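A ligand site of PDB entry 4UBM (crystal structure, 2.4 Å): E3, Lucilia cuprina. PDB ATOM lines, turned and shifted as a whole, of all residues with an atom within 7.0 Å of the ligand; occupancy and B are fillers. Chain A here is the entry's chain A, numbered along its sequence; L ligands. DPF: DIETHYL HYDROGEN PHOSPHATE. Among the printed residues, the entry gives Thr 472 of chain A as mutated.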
ATOM      1  N   HIS A 134      15.061 -18.298   1.255  1.00  0.00           N
ATOM      2  CA  HIS A 134      15.700 -19.556   1.609  1.00  0.00           C
ATOM      3  C   HIS A 134      15.481 -19.903   3.084  1.00  0.00           C
ATOM      4  O   HIS A 134      15.193 -19.033   3.913  1.00  0.00           O
ATOM      5  CB  HIS A 134      17.183 -19.517   1.268  1.00  0.00           C
ATOM      6  CG  HIS A 134      17.982 -18.616   2.168  1.00  0.00           C
ATOM      7  ND1 HIS A 134      18.534 -19.045   3.354  1.00  0.00           N
ATOM      8  CD2 HIS A 134      18.299 -17.308   2.047  1.00  0.00           C
ATOM      9  CE1 HIS A 134      19.167 -18.045   3.931  1.00  0.00           C
ATOM     10  NE2 HIS A 134      19.047 -16.978   3.160  1.00  0.00           N
ATOM     11  N   GLY A 135      15.584 -21.191   3.394  1.00  0.00           N
ATOM     12  CA  GLY A 135      15.481 -21.675   4.750  1.00  0.00           C
ATOM     13  C   GLY A 135      16.881 -21.956   5.247  1.00  0.00           C
ATOM     14  O   GLY A 135      17.855 -21.527   4.629  1.00  0.00           O
ATOM     15  N   GLY A 136      16.977 -22.678   6.348  1.00  0.00           N
ATOM     16  CA  GLY A 136      18.253 -22.897   6.995  1.00  0.00           C
ATOM     17  C   GLY A 136      18.183 -22.475   8.460  1.00  0.00           C
ATOM     18  O   GLY A 136      19.146 -21.963   9.014  1.00  0.00           O
ATOM     19  N   GLY A 137      17.014 -22.712   9.060  1.00  0.00           N
ATOM     20  CA  GLY A 137      16.759 -22.455  10.460  1.00  0.00           C
ATOM     21  C   GLY A 137      17.214 -21.091  10.947  1.00  0.00           C
ATOM     22  O   GLY A 137      17.609 -20.958  12.111  1.00  0.00           O
ATOM     23  N   PHE A 138      17.186 -20.098  10.051  1.00  0.00           N
ATOM     24  CA  PHE A 138      17.691 -18.754  10.333  1.00  0.00           C
ATOM     25  C   PHE A 138      19.180 -18.700  10.712  1.00  0.00           C
ATOM     26  O   PHE A 138      19.643 -17.686  11.221  1.00  0.00           O
ATOM     27  CB  PHE A 138      16.855 -18.083  11.435  1.00  0.00           C
ATOM     28  CG  PHE A 138      15.389 -18.035  11.138  1.00  0.00           C
ATOM     29  CD1 PHE A 138      14.887 -17.130  10.229  1.00  0.00           C
ATOM     30  CD2 PHE A 138      14.516 -18.931  11.755  1.00  0.00           C
ATOM     31  CE1 PHE A 138      13.526 -17.105   9.940  1.00  0.00           C
ATOM     32  CE2 PHE A 138      13.176 -18.907  11.479  1.00  0.00           C
ATOM     33  CZ  PHE A 138      12.678 -17.989  10.581  1.00  0.00           C
ATOM     34  N   ILE A 140      21.750 -20.745   8.542  1.00  0.00           N
ATOM     35  CA  ILE A 140      22.540 -20.961   7.318  1.00  0.00           C
ATOM     36  C   ILE A 140      21.668 -20.672   6.095  1.00  0.00           C
ATOM     37  O   ILE A 140      20.464 -20.437   6.239  1.00  0.00           O
ATOM     38  CB  ILE A 140      23.096 -22.396   7.177  1.00  0.00           C
ATOM     39  CG1 ILE A 140      21.953 -23.399   6.964  1.00  0.00           C
ATOM     40  CG2 ILE A 140      24.033 -22.742   8.331  1.00  0.00           C
ATOM     41  CD1 ILE A 140      22.413 -24.809   6.666  1.00  0.00           C
ATOM     42  N   TYR A 165      19.291 -12.435   3.849  1.00  0.00           N
ATOM     43  CA  TYR A 165      18.951 -11.712   5.059  1.00  0.00           C
ATOM     44  C   TYR A 165      19.939 -12.117   6.182  1.00  0.00           C
ATOM     45  O   TYR A 165      20.540 -13.172   6.098  1.00  0.00           O
ATOM     46  CB  TYR A 165      17.489 -11.984   5.461  1.00  0.00           C
ATOM     47  CG  TYR A 165      17.164 -13.453   5.627  1.00  0.00           C
ATOM     48  CD1 TYR A 165      16.838 -14.264   4.526  1.00  0.00           C
ATOM     49  CD2 TYR A 165      17.193 -14.045   6.896  1.00  0.00           C
ATOM     50  CE1 TYR A 165      16.559 -15.629   4.685  1.00  0.00           C
ATOM     51  CE2 TYR A 165      16.909 -15.400   7.065  1.00  0.00           C
ATOM     52  CZ  TYR A 165      16.595 -16.185   5.955  1.00  0.00           C
ATOM     53  OH  TYR A 165      16.330 -17.519   6.156  1.00  0.00           O
ATOM     54  N   GLU A 217      10.916 -22.416   1.874  1.00  0.00           N
ATOM     55  CA  GLU A 217      10.918 -23.749   2.473  1.00  0.00           C
ATOM     56  C   GLU A 217      11.571 -23.698   3.883  1.00  0.00           C
ATOM     57  O   GLU A 217      12.551 -22.972   4.108  1.00  0.00           O
ATOM     58  CB  GLU A 217      11.643 -24.718   1.534  1.00  0.00           C
ATOM     59  CG  GLU A 217      11.652 -26.185   1.936  1.00  0.00           C
ATOM     60  CD  GLU A 217      12.872 -26.570   2.761  1.00  0.00           C
ATOM     61  OE1 GLU A 217      13.948 -25.918   2.609  1.00  0.00           O
ATOM     62  OE2 GLU A 217      12.759 -27.530   3.563  1.00  0.00           O
ATOM     63  N   SER A 218      10.997 -24.457   4.827  1.00  0.00           N
ATOM     64  CA  SER A 218      11.520 -24.557   6.201  1.00  0.00           C
ATOM     65  C   SER A 218      11.476 -23.194   6.912  1.00  0.00           C
ATOM     66  O   SER A 218      10.393 -22.628   7.096  1.00  0.00           O
ATOM     67  CB  SER A 218      12.952 -25.110   6.194  1.00  0.00           C
ATOM     68  OG  SER A 218      13.260 -25.804   7.400  1.00  0.00           O
ATOM     69  N   ALA A 219      12.649 -22.672   7.266  1.00  0.00           N
ATOM     70  CA  ALA A 219      12.773 -21.330   7.852  1.00  0.00           C
ATOM     71  C   ALA A 219      12.280 -20.266   6.889  1.00  0.00           C
ATOM     72  O   ALA A 219      11.824 -19.208   7.310  1.00  0.00           O
ATOM     73  CB  ALA A 219      14.193 -21.031   8.253  1.00  0.00           C
ATOM     74  N   GLY A 220      12.375 -20.566   5.586  1.00  0.00           N
ATOM     75  CA  GLY A 220      11.910 -19.657   4.562  1.00  0.00           C
ATOM     76  C   GLY A 220      10.394 -19.591   4.550  1.00  0.00           C
ATOM     77  O   GLY A 220       9.814 -18.539   4.283  1.00  0.00           O
ATOM     78  N   ALA A 221       9.751 -20.719   4.837  1.00  0.00           N
ATOM     79  CA  ALA A 221       8.304 -20.765   4.961  1.00  0.00           C
ATOM     80  C   ALA A 221       7.852 -19.923   6.170  1.00  0.00           C
ATOM     81  O   ALA A 221       6.908 -19.137   6.065  1.00  0.00           O
ATOM     82  CB  ALA A 221       7.824 -22.211   5.081  1.00  0.00           C
ATOM     83  N   SER A 244       6.597 -26.684   3.928  1.00  0.00           N
ATOM     84  CA  SER A 244       7.139 -27.354   5.110  1.00  0.00           C
ATOM     85  C   SER A 244       7.482 -26.373   6.229  1.00  0.00           C
ATOM     86  O   SER A 244       8.580 -26.403   6.760  1.00  0.00           O
ATOM     87  CB  SER A 244       8.383 -28.184   4.767  1.00  0.00           C
ATOM     88  OG  SER A 244       8.061 -29.292   3.929  1.00  0.00           O
ATOM     89  N   TRP A 251       9.956 -24.523  16.335  1.00  0.00           N
ATOM     90  CA  TRP A 251      11.321 -24.105  16.044  1.00  0.00           C
ATOM     91  C   TRP A 251      11.421 -22.700  15.439  1.00  0.00           C
ATOM     92  O   TRP A 251      12.511 -22.240  15.133  1.00  0.00           O
ATOM     93  CB  TRP A 251      11.994 -25.096  15.078  1.00  0.00           C
ATOM     94  CG  TRP A 251      11.120 -25.439  13.895  1.00  0.00           C
ATOM     95  CD1 TRP A 251      10.247 -26.499  13.788  1.00  0.00           C
ATOM     96  CD2 TRP A 251      10.991 -24.698  12.676  1.00  0.00           C
ATOM     97  NE1 TRP A 251       9.605 -26.463  12.580  1.00  0.00           N
ATOM     98  CE2 TRP A 251      10.042 -25.369  11.866  1.00  0.00           C
ATOM     99  CE3 TRP A 251      11.594 -23.529  12.179  1.00  0.00           C
ATOM    100  CZ2 TRP A 251       9.673 -24.908  10.607  1.00  0.00           C
ATOM    101  CZ3 TRP A 251      11.221 -23.082  10.910  1.00  0.00           C
ATOM    102  CH2 TRP A 251      10.273 -23.770  10.141  1.00  0.00           C
ATOM    103  N   MET A 308      15.692 -25.519  19.483  1.00  0.00           N
ATOM    104  CA  MET A 308      16.531 -25.953  18.374  1.00  0.00           C
ATOM    105  C   MET A 308      17.635 -24.951  18.044  1.00  0.00           C
ATOM    106  O   MET A 308      18.755 -25.326  17.667  1.00  0.00           O
ATOM    107  CB  MET A 308      15.630 -26.213  17.154  1.00  0.00           C
ATOM    108  CG  MET A 308      16.365 -26.729  15.940  1.00  0.00           C
ATOM    109  SD  MET A 308      15.256 -27.335  14.646  1.00  0.00           S
ATOM    110  CE  MET A 308      14.726 -28.898  15.349  1.00  0.00           C
ATOM    111  N   PHE A 309      17.327 -23.669  18.178  1.00  0.00           N
ATOM    112  CA  PHE A 309      18.274 -22.617  17.882  1.00  0.00           C
ATOM    113  C   PHE A 309      18.302 -21.586  19.009  1.00  0.00           C
ATOM    114  O   PHE A 309      17.250 -21.224  19.539  1.00  0.00           O
ATOM    115  CB  PHE A 309      17.937 -21.945  16.561  1.00  0.00           C
ATOM    116  CG  PHE A 309      17.784 -22.898  15.410  1.00  0.00           C
ATOM    117  CD1 PHE A 309      18.876 -23.627  14.939  1.00  0.00           C
ATOM    118  CD2 PHE A 309      16.560 -23.066  14.794  1.00  0.00           C
ATOM    119  CE1 PHE A 309      18.730 -24.516  13.859  1.00  0.00           C
ATOM    120  CE2 PHE A 309      16.404 -23.959  13.723  1.00  0.00           C
ATOM    121  CZ  PHE A 309      17.505 -24.683  13.253  1.00  0.00           C
ATOM    122  N   PHE A 354      14.595 -36.440   7.780  1.00  0.00           N
ATOM    123  CA  PHE A 354      15.692 -35.506   7.896  1.00  0.00           C
ATOM    124  C   PHE A 354      16.601 -35.773   9.104  1.00  0.00           C
ATOM    125  O   PHE A 354      17.807 -35.512   9.066  1.00  0.00           O
ATOM    126  CB  PHE A 354      15.128 -34.081   7.975  1.00  0.00           C
ATOM    127  CG  PHE A 354      16.175 -33.012   7.917  1.00  0.00           C
ATOM    128  CD1 PHE A 354      16.711 -32.501   9.081  1.00  0.00           C
ATOM    129  CD2 PHE A 354      16.616 -32.523   6.696  1.00  0.00           C
ATOM    130  CE1 PHE A 354      17.681 -31.514   9.034  1.00  0.00           C
ATOM    131  CE2 PHE A 354      17.572 -31.531   6.646  1.00  0.00           C
ATOM    132  CZ  PHE A 354      18.111 -31.029   7.821  1.00  0.00           C
ATOM    133  N   PHE A 355      16.012 -36.300  10.181  1.00  0.00           N
ATOM    134  CA  PHE A 355      16.717 -36.435  11.453  1.00  0.00           C
ATOM    135  C   PHE A 355      17.519 -37.733  11.622  1.00  0.00           C
ATOM    136  O   PHE A 355      18.008 -38.023  12.712  1.00  0.00           O
ATOM    137  CB  PHE A 355      15.731 -36.302  12.608  1.00  0.00           C
ATOM    138  CG  PHE A 355      15.095 -34.947  12.698  1.00  0.00           C
ATOM    139  CD1 PHE A 355      15.677 -33.939  13.449  1.00  0.00           C
ATOM    140  CD2 PHE A 355      13.941 -34.655  11.977  1.00  0.00           C
ATOM    141  CE1 PHE A 355      15.108 -32.680  13.501  1.00  0.00           C
ATOM    142  CE2 PHE A 355      13.363 -33.400  12.028  1.00  0.00           C
ATOM    143  CZ  PHE A 355      13.942 -32.414  12.789  1.00  0.00           C
ATOM    144  N   TYR A 420       7.279 -31.188  14.471  1.00  0.00           N
ATOM    145  CA  TYR A 420       7.873 -30.039  13.801  1.00  0.00           C
ATOM    146  C   TYR A 420       7.082 -29.500  12.604  1.00  0.00           C
ATOM    147  O   TYR A 420       7.268 -28.342  12.233  1.00  0.00           O
ATOM    148  CB  TYR A 420       9.291 -30.383  13.319  1.00  0.00           C
ATOM    149  CG  TYR A 420      10.270 -30.662  14.447  1.00  0.00           C
ATOM    150  CD1 TYR A 420      10.667 -29.641  15.310  1.00  0.00           C
ATOM    151  CD2 TYR A 420      10.796 -31.926  14.631  1.00  0.00           C
ATOM    152  CE1 TYR A 420      11.572 -29.891  16.354  1.00  0.00           C
ATOM    153  CE2 TYR A 420      11.693 -32.181  15.664  1.00  0.00           C
ATOM    154  CZ  TYR A 420      12.082 -31.164  16.516  1.00  0.00           C
ATOM    155  OH  TYR A 420      12.973 -31.423  17.528  1.00  0.00           O
ATOM    156  N   PHE A 421       6.212 -30.305  11.993  1.00  0.00           N
ATOM    157  CA  PHE A 421       5.584 -29.857  10.754  1.00  0.00           C
ATOM    158  C   PHE A 421       4.067 -30.034  10.678  1.00  0.00           C
ATOM    159  O   PHE A 421       3.335 -29.043  10.500  1.00  0.00           O
ATOM    160  CB  PHE A 421       6.251 -30.560   9.555  1.00  0.00           C
ATOM    161  CG  PHE A 421       7.727 -30.226   9.406  1.00  0.00           C
ATOM    162  CD1 PHE A 421       8.128 -28.952   9.036  1.00  0.00           C
ATOM    163  CD2 PHE A 421       8.696 -31.183   9.652  1.00  0.00           C
ATOM    164  CE1 PHE A 421       9.464 -28.636   8.926  1.00  0.00           C
ATOM    165  CE2 PHE A 421      10.047 -30.873   9.534  1.00  0.00           C
ATOM    166  CZ  PHE A 421      10.428 -29.606   9.171  1.00  0.00           C
ATOM    167  N   TYR A 457      21.498 -30.510   0.860  1.00  0.00           N
ATOM    168  CA  TYR A 457      20.899 -30.872   2.143  1.00  0.00           C
ATOM    169  C   TYR A 457      20.934 -32.375   2.398  1.00  0.00           C
ATOM    170  O   TYR A 457      20.930 -32.809   3.535  1.00  0.00           O
ATOM    171  CB  TYR A 457      19.465 -30.367   2.222  1.00  0.00           C
ATOM    172  CG  TYR A 457      19.344 -28.912   2.613  1.00  0.00           C
ATOM    173  CD1 TYR A 457      19.605 -28.496   3.909  1.00  0.00           C
ATOM    174  CD2 TYR A 457      18.945 -27.959   1.679  1.00  0.00           C
ATOM    175  CE1 TYR A 457      19.471 -27.167   4.282  1.00  0.00           C
ATOM    176  CE2 TYR A 457      18.819 -26.617   2.043  1.00  0.00           C
ATOM    177  CZ  TYR A 457      19.082 -26.233   3.340  1.00  0.00           C
ATOM    178  OH  TYR A 457      18.960 -24.900   3.695  1.00  0.00           O
ATOM    179  N   MET A 460      24.008 -33.260   4.336  1.00  0.00           N
ATOM    180  CA  MET A 460      23.957 -32.868   5.744  1.00  0.00           C
ATOM    181  C   MET A 460      23.108 -33.821   6.580  1.00  0.00           C
ATOM    182  O   MET A 460      23.519 -34.216   7.671  1.00  0.00           O
ATOM    183  CB  MET A 460      23.409 -31.443   5.865  1.00  0.00           C
ATOM    184  CG  MET A 460      23.159 -30.998   7.301  1.00  0.00           C
ATOM    185  SD  MET A 460      21.985 -29.635   7.405  1.00  0.00           S
ATOM    186  CE  MET A 460      22.678 -28.509   6.195  1.00  0.00           C
ATOM    187  N   HIS A 471      12.301 -34.018   4.399  1.00  0.00           N
ATOM    188  CA  HIS A 471      12.333 -32.575   4.370  1.00  0.00           C
ATOM    189  C   HIS A 471      13.474 -32.067   3.443  1.00  0.00           C
ATOM    190  O   HIS A 471      14.580 -32.613   3.485  1.00  0.00           O
ATOM    191  CB  HIS A 471      12.500 -32.085   5.810  1.00  0.00           C
ATOM    192  CG  HIS A 471      12.459 -30.602   5.950  1.00  0.00           C
ATOM    193  ND1 HIS A 471      11.276 -29.884   5.881  1.00  0.00           N
ATOM    194  CD2 HIS A 471      13.448 -29.694   6.131  1.00  0.00           C
ATOM    195  CE1 HIS A 471      11.552 -28.599   6.037  1.00  0.00           C
ATOM    196  NE2 HIS A 471      12.855 -28.456   6.181  1.00  0.00           N
ATOM    197  N   THR A 472      13.173 -31.067   2.604  1.00  0.00           N
ATOM    198  CA  THR A 472      14.077 -30.477   1.575  1.00  0.00           C
ATOM    199  C   THR A 472      14.305 -31.313   0.321  1.00  0.00           C
ATOM    200  O   THR A 472      14.989 -30.863  -0.597  1.00  0.00           O
ATOM    201  CB  THR A 472      15.522 -30.138   2.070  1.00  0.00           C
ATOM    202  OG1 THR A 472      16.282 -31.348   2.209  1.00  0.00           O
ATOM    203  CG2 THR A 472      15.518 -29.331   3.351  1.00  0.00           C
ATOM    204  N   LEU A 475      13.231 -29.365  -2.951  1.00  0.00           N
ATOM    205  CA  LEU A 475      13.985 -28.237  -3.473  1.00  0.00           C
ATOM    206  C   LEU A 475      14.681 -28.594  -4.779  1.00  0.00           C
ATOM    207  O   LEU A 475      14.842 -27.752  -5.661  1.00  0.00           O
ATOM    208  CB  LEU A 475      15.034 -27.778  -2.468  1.00  0.00           C
ATOM    209  CG  LEU A 475      14.465 -27.056  -1.245  1.00  0.00           C
ATOM    210  CD1 LEU A 475      15.581 -26.640  -0.288  1.00  0.00           C
ATOM    211  CD2 LEU A 475      13.603 -25.869  -1.672  1.00  0.00           C
HETATM  212  O4  DPF L   1      14.971 -24.120   7.804  1.00  0.00           O
HETATM  213  P1  DPF L   1      14.523 -25.512   8.150  1.00  0.00           P
HETATM  214  O3  DPF L   1      14.473 -25.592   9.806  1.00  0.00           O
HETATM  215  C1  DPF L   1      13.321 -26.105  10.387  1.00  0.00           C
HETATM  216  C4  DPF L   1      13.702 -27.287  11.255  1.00  0.00           C
HETATM  217  O1  DPF L   1      15.815 -26.485   7.799  1.00  0.00           O
HETATM  218  C2  DPF L   1      15.992 -26.850   6.491  1.00  0.00           C
HETATM  219  C3  DPF L   1      16.809 -28.117   6.479  1.00  0.00           C
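The backbone NH of Gly 136 lies within hydrogen-bond range of an oxygen (O4) of the ligand (2.9 Å).
N of Gly 137 lies within hydrogen-bond range of O4 of the ligand, 2.8 Å away.
An oxygen (O4) of the ligand lies within hydrogen-bond range of the backbone NH (N) of Ala 219 (2.8 Å).
P1 of the ligand is bonded to OG of Ser 218 (1.5 Å).
The indole nitrogen (NE1) of Trp 251 sits at hydrogen-bond distance from the backbone carbonyl oxygen (O) of Tyr 420, at 3.0 Å.
The side-chain carboxylate (OE2) of Glu 217 sits at hydrogen-bond distance from a ring nitrogen (NE2) of His 471.
The side-chain hydroxyl of Ser 218 is in hydrogen-bond range of a ring nitrogen (NE2) of His 471 (2.9 Å).
Merely in contact with the ligand: Gly 135 (3.9 Å), Trp 251 (3.6 Å), Met 308 (3.7 Å), Phe 354 (3.5 Å), Tyr 457 (3.6 Å), His 471 (3.5 Å) and Thr 472 (3.6 Å).
11 residues have an atom within 4 Å of the ligand: Gly 135, Gly 136, Gly 137, Ser 218, Ala 219, Trp 251, Met 308, Phe 354, Tyr 457, His 471 and Thr 472.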
